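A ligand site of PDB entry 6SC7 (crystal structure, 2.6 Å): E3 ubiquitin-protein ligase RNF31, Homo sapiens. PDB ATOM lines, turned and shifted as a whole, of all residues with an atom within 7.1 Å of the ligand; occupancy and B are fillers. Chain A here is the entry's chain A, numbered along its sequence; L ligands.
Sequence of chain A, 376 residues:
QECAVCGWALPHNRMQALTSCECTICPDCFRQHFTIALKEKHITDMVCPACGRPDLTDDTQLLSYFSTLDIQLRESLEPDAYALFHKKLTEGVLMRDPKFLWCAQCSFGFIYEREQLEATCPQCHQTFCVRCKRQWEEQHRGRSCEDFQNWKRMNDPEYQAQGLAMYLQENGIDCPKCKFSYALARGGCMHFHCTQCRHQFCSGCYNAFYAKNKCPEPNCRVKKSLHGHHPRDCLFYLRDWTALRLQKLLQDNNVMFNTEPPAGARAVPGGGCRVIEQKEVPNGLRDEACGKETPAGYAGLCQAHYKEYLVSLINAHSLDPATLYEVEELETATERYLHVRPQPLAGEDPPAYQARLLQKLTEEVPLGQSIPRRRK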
ATOM      1  N   ILE A 173     -30.299  10.203  -5.988  1.00  0.00           N
ATOM      2  CA  ILE A 173     -30.758  10.353  -4.614  1.00  0.00           C
ATOM      3  C   ILE A 173     -29.864  11.387  -3.938  1.00  0.00           C
ATOM      4  O   ILE A 173     -28.686  11.121  -3.675  1.00  0.00           O
ATOM      5  CB  ILE A 173     -30.737   9.024  -3.853  1.00  0.00           C
ATOM      6  CG1 ILE A 173     -31.665   8.006  -4.532  1.00  0.00           C
ATOM      7  CG2 ILE A 173     -31.144   9.225  -2.405  1.00  0.00           C
ATOM      8  CD1 ILE A 173     -31.690   6.656  -3.858  1.00  0.00           C
ATOM      9  N   TYR A 182     -26.252  10.595  -5.105  1.00  0.00           N
ATOM     10  CA  TYR A 182     -26.045   9.170  -5.352  1.00  0.00           C
ATOM     11  C   TYR A 182     -26.755   8.803  -6.649  1.00  0.00           C
ATOM     12  O   TYR A 182     -27.989   8.881  -6.719  1.00  0.00           O
ATOM     13  CB  TYR A 182     -26.559   8.318  -4.201  1.00  0.00           C
ATOM     14  CG  TYR A 182     -25.910   8.585  -2.865  1.00  0.00           C
ATOM     15  CD1 TYR A 182     -26.419   9.549  -2.002  1.00  0.00           C
ATOM     16  CD2 TYR A 182     -24.789   7.865  -2.451  1.00  0.00           C
ATOM     17  CE1 TYR A 182     -25.825   9.798  -0.774  1.00  0.00           C
ATOM     18  CE2 TYR A 182     -24.198   8.110  -1.233  1.00  0.00           C
ATOM     19  CZ  TYR A 182     -24.718   9.075  -0.398  1.00  0.00           C
ATOM     20  OH  TYR A 182     -24.128   9.320   0.820  1.00  0.00           O
ATOM     21  N   LEU A 184     -28.165   6.421  -8.089  1.00  0.00           N
ATOM     22  CA  LEU A 184     -28.754   5.120  -7.805  1.00  0.00           C
ATOM     23  C   LEU A 184     -30.269   5.186  -7.984  1.00  0.00           C
ATOM     24  O   LEU A 184     -30.852   6.268  -8.065  1.00  0.00           O
ATOM     25  CB  LEU A 184     -28.421   4.652  -6.386  1.00  0.00           C
ATOM     26  CG  LEU A 184     -26.941   4.524  -6.022  1.00  0.00           C
ATOM     27  CD1 LEU A 184     -26.779   4.623  -4.520  1.00  0.00           C
ATOM     28  CD2 LEU A 184     -26.379   3.218  -6.547  1.00  0.00           C
ATOM     29  N   ALA A 185     -30.883   4.020  -8.034  1.00  0.00           N
ATOM     30  CA  ALA A 185     -32.323   3.884  -8.047  1.00  0.00           C
ATOM     31  C   ALA A 185     -32.824   3.523  -6.644  1.00  0.00           C
ATOM     32  O   ALA A 185     -32.132   2.856  -5.881  1.00  0.00           O
ATOM     33  CB  ALA A 185     -32.779   2.825  -9.052  1.00  0.00           C
ATOM     34  N   ARG A 186     -34.038   3.975  -6.334  1.00  0.00           N
ATOM     35  CA  ARG A 186     -34.588   3.722  -5.006  1.00  0.00           C
ATOM     36  C   ARG A 186     -34.965   2.252  -4.828  1.00  0.00           C
ATOM     37  O   ARG A 186     -34.681   1.648  -3.795  1.00  0.00           O
ATOM     38  CB  ARG A 186     -35.797   4.630  -4.758  1.00  0.00           C
ATOM     39  CG  ARG A 186     -35.469   6.110  -4.818  1.00  0.00           C
ATOM     40  CD  ARG A 186     -36.456   6.873  -5.678  1.00  0.00           C
ATOM     41  NE  ARG A 186     -36.279   8.313  -5.547  1.00  0.00           N
ATOM     42  CZ  ARG A 186     -35.358   9.021  -6.187  1.00  0.00           C
ATOM     43  NH1 ARG A 186     -35.272  10.330  -6.008  1.00  0.00           N
ATOM     44  NH2 ARG A 186     -34.523   8.424  -7.031  1.00  0.00           N
ATOM     45  N   GLY A 188     -37.089  -0.923  -3.954  1.00  0.00           N
ATOM     46  CA  GLY A 188     -38.152  -1.217  -3.017  1.00  0.00           C
ATOM     47  C   GLY A 188     -37.908  -0.671  -1.628  1.00  0.00           C
ATOM     48  O   GLY A 188     -38.863  -0.410  -0.877  1.00  0.00           O
ATOM     49  N   CYS A 189     -36.642  -0.498  -1.274  1.00  0.00           N
ATOM     50  CA  CYS A 189     -36.274  -0.011   0.052  1.00  0.00           C
ATOM     51  C   CYS A 189     -36.249   1.516   0.042  1.00  0.00           C
ATOM     52  O   CYS A 189     -35.501   2.122  -0.730  1.00  0.00           O
ATOM     53  CB  CYS A 189     -34.917  -0.564   0.481  1.00  0.00           C
ATOM     54  SG  CYS A 189     -34.386  -0.054   2.129  1.00  0.00           S
ATOM     55  N   MET A 190     -37.069   2.128   0.897  1.00  0.00           N
ATOM     56  CA  MET A 190     -37.170   3.576   0.978  1.00  0.00           C
ATOM     57  C   MET A 190     -36.267   4.176   2.045  1.00  0.00           C
ATOM     58  O   MET A 190     -35.927   5.362   1.949  1.00  0.00           O
ATOM     59  CB  MET A 190     -38.616   3.991   1.249  1.00  0.00           C
ATOM     60  CG  MET A 190     -39.642   3.385   0.303  1.00  0.00           C
ATOM     61  SD  MET A 190     -39.348   3.821  -1.429  1.00  0.00           S
ATOM     62  CE  MET A 190     -39.380   5.609  -1.327  1.00  0.00           C
ATOM     63  N   HIS A 191     -35.879   3.405   3.050  1.00  0.00           N
ATOM     64  CA  HIS A 191     -35.042   3.901   4.146  1.00  0.00           C
ATOM     65  C   HIS A 191     -33.606   4.020   3.666  1.00  0.00           C
ATOM     66  O   HIS A 191     -32.921   3.004   3.488  1.00  0.00           O
ATOM     67  CB  HIS A 191     -35.158   2.982   5.352  1.00  0.00           C
ATOM     68  CG  HIS A 191     -34.492   3.514   6.586  1.00  0.00           C
ATOM     69  ND1 HIS A 191     -34.508   2.836   7.789  1.00  0.00           N
ATOM     70  CD2 HIS A 191     -33.800   4.657   6.805  1.00  0.00           C
ATOM     71  CE1 HIS A 191     -33.852   3.538   8.693  1.00  0.00           C
ATOM     72  NE2 HIS A 191     -33.414   4.647   8.119  1.00  0.00           N
ATOM     73  N   PHE A 192     -33.138   5.247   3.458  1.00  0.00           N
ATOM     74  CA  PHE A 192     -31.797   5.503   2.945  1.00  0.00           C
ATOM     75  C   PHE A 192     -30.875   5.954   4.068  1.00  0.00           C
ATOM     76  O   PHE A 192     -31.294   6.690   4.977  1.00  0.00           O
ATOM     77  CB  PHE A 192     -31.831   6.555   1.843  1.00  0.00           C
ATOM     78  CG  PHE A 192     -30.636   6.511   0.928  1.00  0.00           C
ATOM     79  CD1 PHE A 192     -30.657   5.728  -0.216  1.00  0.00           C
ATOM     80  CD2 PHE A 192     -29.505   7.249   1.216  1.00  0.00           C
ATOM     81  CE1 PHE A 192     -29.561   5.677  -1.055  1.00  0.00           C
ATOM     82  CE2 PHE A 192     -28.409   7.207   0.375  1.00  0.00           C
ATOM     83  CZ  PHE A 192     -28.440   6.424  -0.766  1.00  0.00           C
ATOM     84  N   HIS A 193     -29.624   5.511   4.012  1.00  0.00           N
ATOM     85  CA  HIS A 193     -28.588   5.899   4.964  1.00  0.00           C
ATOM     86  C   HIS A 193     -27.457   6.572   4.206  1.00  0.00           C
ATOM     87  O   HIS A 193     -26.874   5.969   3.296  1.00  0.00           O
ATOM     88  CB  HIS A 193     -28.053   4.682   5.738  1.00  0.00           C
ATOM     89  CG  HIS A 193     -29.092   3.989   6.568  1.00  0.00           C
ATOM     90  ND1 HIS A 193     -29.933   3.030   6.048  1.00  0.00           N
ATOM     91  CD2 HIS A 193     -29.418   4.121   7.871  1.00  0.00           C
ATOM     92  CE1 HIS A 193     -30.740   2.593   7.011  1.00  0.00           C
ATOM     93  NE2 HIS A 193     -30.442   3.238   8.127  1.00  0.00           N
ATOM     94  N   CYS A 194     -27.161   7.821   4.560  1.00  0.00           N
ATOM     95  CA  CYS A 194     -26.070   8.564   3.941  1.00  0.00           C
ATOM     96  C   CYS A 194     -24.776   8.232   4.658  1.00  0.00           C
ATOM     97  O   CYS A 194     -24.663   8.435   5.871  1.00  0.00           O
ATOM     98  CB  CYS A 194     -26.351  10.062   3.975  1.00  0.00           C
ATOM     99  SG  CYS A 194     -25.101  11.055   3.122  1.00  0.00           S
ATOM    100  N   THR A 195     -23.783   7.734   3.908  1.00  0.00           N
ATOM    101  CA  THR A 195     -22.511   7.376   4.518  1.00  0.00           C
ATOM    102  C   THR A 195     -21.676   8.609   4.874  1.00  0.00           C
ATOM    103  O   THR A 195     -20.735   8.495   5.669  1.00  0.00           O
ATOM    104  CB  THR A 195     -21.717   6.472   3.584  1.00  0.00           C
ATOM    105  OG1 THR A 195     -21.623   7.075   2.284  1.00  0.00           O
ATOM    106  CG2 THR A 195     -22.397   5.117   3.458  1.00  0.00           C
ATOM    107  N   GLN A 196     -21.990   9.767   4.305  1.00  0.00           N
ATOM    108  CA  GLN A 196     -21.193  10.968   4.540  1.00  0.00           C
ATOM    109  C   GLN A 196     -21.607  11.702   5.812  1.00  0.00           C
ATOM    110  O   GLN A 196     -20.742  12.238   6.519  1.00  0.00           O
ATOM    111  CB  GLN A 196     -21.301  11.907   3.339  1.00  0.00           C
ATOM    112  CG  GLN A 196     -20.455  13.161   3.456  1.00  0.00           C
ATOM    113  CD  GLN A 196     -20.047  13.730   2.108  1.00  0.00           C
ATOM    114  OE1 GLN A 196     -20.832  14.433   1.460  1.00  0.00           O
ATOM    115  NE2 GLN A 196     -18.820  13.444   1.687  1.00  0.00           N
ATOM    116  N   PHE A 201     -33.090   9.138   5.836  1.00  0.00           N
ATOM    117  CA  PHE A 201     -34.208   9.796   5.192  1.00  0.00           C
ATOM    118  C   PHE A 201     -34.853   8.835   4.195  1.00  0.00           C
ATOM    119  O   PHE A 201     -34.285   7.790   3.859  1.00  0.00           O
ATOM    120  CB  PHE A 201     -33.773  11.089   4.496  1.00  0.00           C
ATOM    121  CG  PHE A 201     -32.712  10.882   3.444  1.00  0.00           C
ATOM    122  CD1 PHE A 201     -31.371  10.854   3.806  1.00  0.00           C
ATOM    123  CD2 PHE A 201     -33.051  10.705   2.121  1.00  0.00           C
ATOM    124  CE1 PHE A 201     -30.390  10.659   2.850  1.00  0.00           C
ATOM    125  CE2 PHE A 201     -32.074  10.516   1.153  1.00  0.00           C
ATOM    126  CZ  PHE A 201     -30.743  10.488   1.519  1.00  0.00           C
ATOM    127  N   SER A 203     -35.882   7.998   0.432  1.00  0.00           N
ATOM    128  CA  SER A 203     -35.396   8.338  -0.900  1.00  0.00           C
ATOM    129  C   SER A 203     -36.508   8.767  -1.840  1.00  0.00           C
ATOM    130  O   SER A 203     -36.220   9.121  -2.993  1.00  0.00           O
ATOM    131  CB  SER A 203     -34.645   7.145  -1.497  1.00  0.00           C
ATOM    132  OG  SER A 203     -35.450   5.983  -1.538  1.00  0.00           O
ATOM    133  N   GLU A 277     -27.406  -2.007  -8.482  1.00  0.00           N
ATOM    134  CA  GLU A 277     -27.470  -1.803  -7.038  1.00  0.00           C
ATOM    135  C   GLU A 277     -26.056  -1.841  -6.464  1.00  0.00           C
ATOM    136  O   GLU A 277     -25.106  -2.291  -7.111  1.00  0.00           O
ATOM    137  CB  GLU A 277     -28.354  -2.857  -6.370  1.00  0.00           C
ATOM    138  CG  GLU A 277     -29.695  -3.065  -7.045  1.00  0.00           C
ATOM    139  CD  GLU A 277     -30.693  -3.761  -6.140  1.00  0.00           C
ATOM    140  OE1 GLU A 277     -30.306  -4.755  -5.476  1.00  0.00           O
ATOM    141  OE2 GLU A 277     -31.864  -3.336  -6.098  1.00  0.00           O
ATOM    142  N   GLN A 278     -25.929  -1.367  -5.229  1.00  0.00           N
ATOM    143  CA  GLN A 278     -24.644  -1.326  -4.528  1.00  0.00           C
ATOM    144  C   GLN A 278     -24.730  -2.214  -3.300  1.00  0.00           C
ATOM    145  O   GLN A 278     -25.410  -1.875  -2.325  1.00  0.00           O
ATOM    146  CB  GLN A 278     -24.274   0.106  -4.155  1.00  0.00           C
ATOM    147  CG  GLN A 278     -23.839   0.959  -5.343  1.00  0.00           C
ATOM    148  CD  GLN A 278     -22.789   1.986  -4.977  1.00  0.00           C
ATOM    149  OE1 GLN A 278     -21.987   1.777  -4.069  1.00  0.00           O
ATOM    150  NE2 GLN A 278     -22.793   3.112  -5.685  1.00  0.00           N
ATOM    151  N   LYS A 279     -24.050  -3.358  -3.350  1.00  0.00           N
ATOM    152  CA  LYS A 279     -24.016  -4.306  -2.252  1.00  0.00           C
ATOM    153  C   LYS A 279     -22.711  -4.176  -1.477  1.00  0.00           C
ATOM    154  O   LYS A 279     -21.713  -3.655  -1.968  1.00  0.00           O
ATOM    155  CB  LYS A 279     -24.169  -5.741  -2.780  1.00  0.00           C
ATOM    156  CG  LYS A 279     -25.465  -5.988  -3.529  1.00  0.00           C
ATOM    157  N   GLU A 280     -22.740  -4.654  -0.236  1.00  0.00           N
ATOM    158  CA  GLU A 280     -21.600  -4.533   0.666  1.00  0.00           C
ATOM    159  C   GLU A 280     -20.586  -5.634   0.373  1.00  0.00           C
ATOM    160  O   GLU A 280     -20.922  -6.821   0.399  1.00  0.00           O
ATOM    161  CB  GLU A 280     -22.062  -4.588   2.125  1.00  0.00           C
ATOM    162  CG  GLU A 280     -21.029  -4.093   3.119  1.00  0.00           C
ATOM    163  CD  GLU A 280     -20.771  -2.599   2.992  1.00  0.00           C
ATOM    164  OE1 GLU A 280     -19.626  -2.165   3.247  1.00  0.00           O
ATOM    165  OE2 GLU A 280     -21.720  -1.856   2.659  1.00  0.00           O
ATOM    166  N   LEU A 285     -17.594  -1.142  -1.974  1.00  0.00           N
ATOM    167  CA  LEU A 285     -18.914  -1.429  -2.539  1.00  0.00           C
ATOM    168  C   LEU A 285     -18.748  -1.865  -3.986  1.00  0.00           C
ATOM    169  O   LEU A 285     -18.033  -1.220  -4.759  1.00  0.00           O
ATOM    170  CB  LEU A 285     -19.825  -0.192  -2.450  1.00  0.00           C
ATOM    171  CG  LEU A 285     -20.242   0.217  -1.039  1.00  0.00           C
ATOM    172  CD1 LEU A 285     -20.941   1.574  -1.045  1.00  0.00           C
ATOM    173  CD2 LEU A 285     -21.135  -0.843  -0.421  1.00  0.00           C
HETATM  174  C1  LIG L   1     -27.887   2.379  -0.752  1.00  0.00           C
HETATM  175  C2  LIG L   1     -32.566   1.284   0.773  1.00  0.00           C
HETATM  176  C3  LIG L   1     -31.677  -1.047   1.436  1.00  0.00           C
HETATM  177  C4  LIG L   1     -32.529  -4.250   3.065  1.00  0.00           C
HETATM  178  C5  LIG L   1     -31.928  -4.432   4.465  1.00  0.00           C
HETATM  179  C6  LIG L   1     -29.004  -5.015   2.890  1.00  0.00           C
HETATM  180  C7  LIG L   1     -25.575   2.983  -1.627  1.00  0.00           C
HETATM  181  C8  LIG L   1     -24.448   3.983  -1.442  1.00  0.00           C
HETATM  182  C9  LIG L   1     -23.988   4.070   0.023  1.00  0.00           C
HETATM  183  C10 LIG L   1     -25.151   4.499   0.946  1.00  0.00           C
HETATM  184  C11 LIG L   1     -26.466   3.733   0.630  1.00  0.00           C
HETATM  185  C12 LIG L   1     -26.648   3.051  -0.542  1.00  0.00           C
HETATM  186  C13 LIG L   1     -28.610   3.160   1.413  1.00  0.00           C
HETATM  187  C14 LIG L   1     -28.854   2.441   0.245  1.00  0.00           C
HETATM  188  C15 LIG L   1     -30.198   1.730   0.046  1.00  0.00           C
HETATM  189  C16 LIG L   1     -32.678   0.070   1.707  1.00  0.00           C
HETATM  190  N1  LIG L   1     -27.450   3.773   1.563  1.00  0.00           N
HETATM  191  N2  LIG L   1     -31.301   1.975   0.966  1.00  0.00           N
HETATM  192  O1  LIG L   1     -29.586   3.223   2.414  1.00  0.00           O
HETATM  193  O2  LIG L   1     -30.332   0.963  -0.842  1.00  0.00           O
HETATM  194  C17 LIG L   1     -32.323  -2.439   1.583  1.00  0.00           C
HETATM  195  C18 LIG L   1     -29.671  -3.798   3.535  1.00  0.00           C
HETATM  196  C19 LIG L   1     -27.596  -4.687   2.381  1.00  0.00           C
HETATM  197  C20 LIG L   1     -27.714  -2.623   0.941  1.00  0.00           C
HETATM  198  C21 LIG L   1     -27.235  -0.446   1.708  1.00  0.00           C
HETATM  199  C22 LIG L   1     -25.960   0.359   1.356  1.00  0.00           C
HETATM  200  C23 LIG L   1     -26.264   0.858   4.794  1.00  0.00           C
HETATM  201  C24 LIG L   1     -27.082  -0.326   4.288  1.00  0.00           C
HETATM  202  C25 LIG L   1     -27.897  -0.020   3.021  1.00  0.00           C
HETATM  203  C26 LIG L   1     -24.650  -0.269   1.831  1.00  0.00           C
HETATM  204  C27 LIG L   1     -24.364  -0.036   3.314  1.00  0.00           C
HETATM  205  C28 LIG L   1     -25.047   1.196   3.915  1.00  0.00           C
HETATM  206  N3  LIG L   1     -30.497  -4.206   4.666  1.00  0.00           N
HETATM  207  N4  LIG L   1     -27.644  -4.069   1.076  1.00  0.00           N
HETATM  208  O3  LIG L   1     -32.755  -2.881   2.838  1.00  0.00           O
HETATM  209  O4  LIG L   1     -26.884  -1.812   1.735  1.00  0.00           O
HETATM  210  O5  LIG L   1     -32.463  -3.124   0.622  1.00  0.00           O
HETATM  211  O6  LIG L   1     -32.609  -4.770   5.364  1.00  0.00           O
HETATM  212  O7  LIG L   1     -28.465  -2.133   0.173  1.00  0.00           O
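SG of Cys 189 is covalently linked to C16 of the ligand. O1 of the ligand lies within hydrogen-bond range of N of His 193 (2.8 Å). O of His 193 is in hydrogen-bond range of N1 of the ligand. The backbone carbonyl oxygen of His 191 is in hydrogen-bond range of a nitrogen (N2) of the ligand (3.2 Å).
A ring nitrogen (NE2) of His 191 lies within hydrogen-bond range of a ring nitrogen (NE2) of His 193 (3.3 Å). N of Phe 192 lies within hydrogen-bond range of O of Phe 201, 2.8 Å away. The backbone NH of Thr 195 sits at hydrogen-bond distance from the side-chain hydroxyl of Tyr 182.
CD1 of Leu 184 touches C7 of the ligand, at 3.5 Å. Phe 192 touches the ligand (CA to O1, 3.2 Å). Thr 195 touches the ligand. Gln 278 touches the ligand. Glu 280 touches the ligand. Hydrophobic or aromatic side chains within 4 Å of the ligand: Leu 184, Phe 192 and His 193. Within 4 Å of the ligand: Leu 184, Cys 189, His 191, Phe 192, His 193, Thr 195, Gln 278 and Glu 280.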
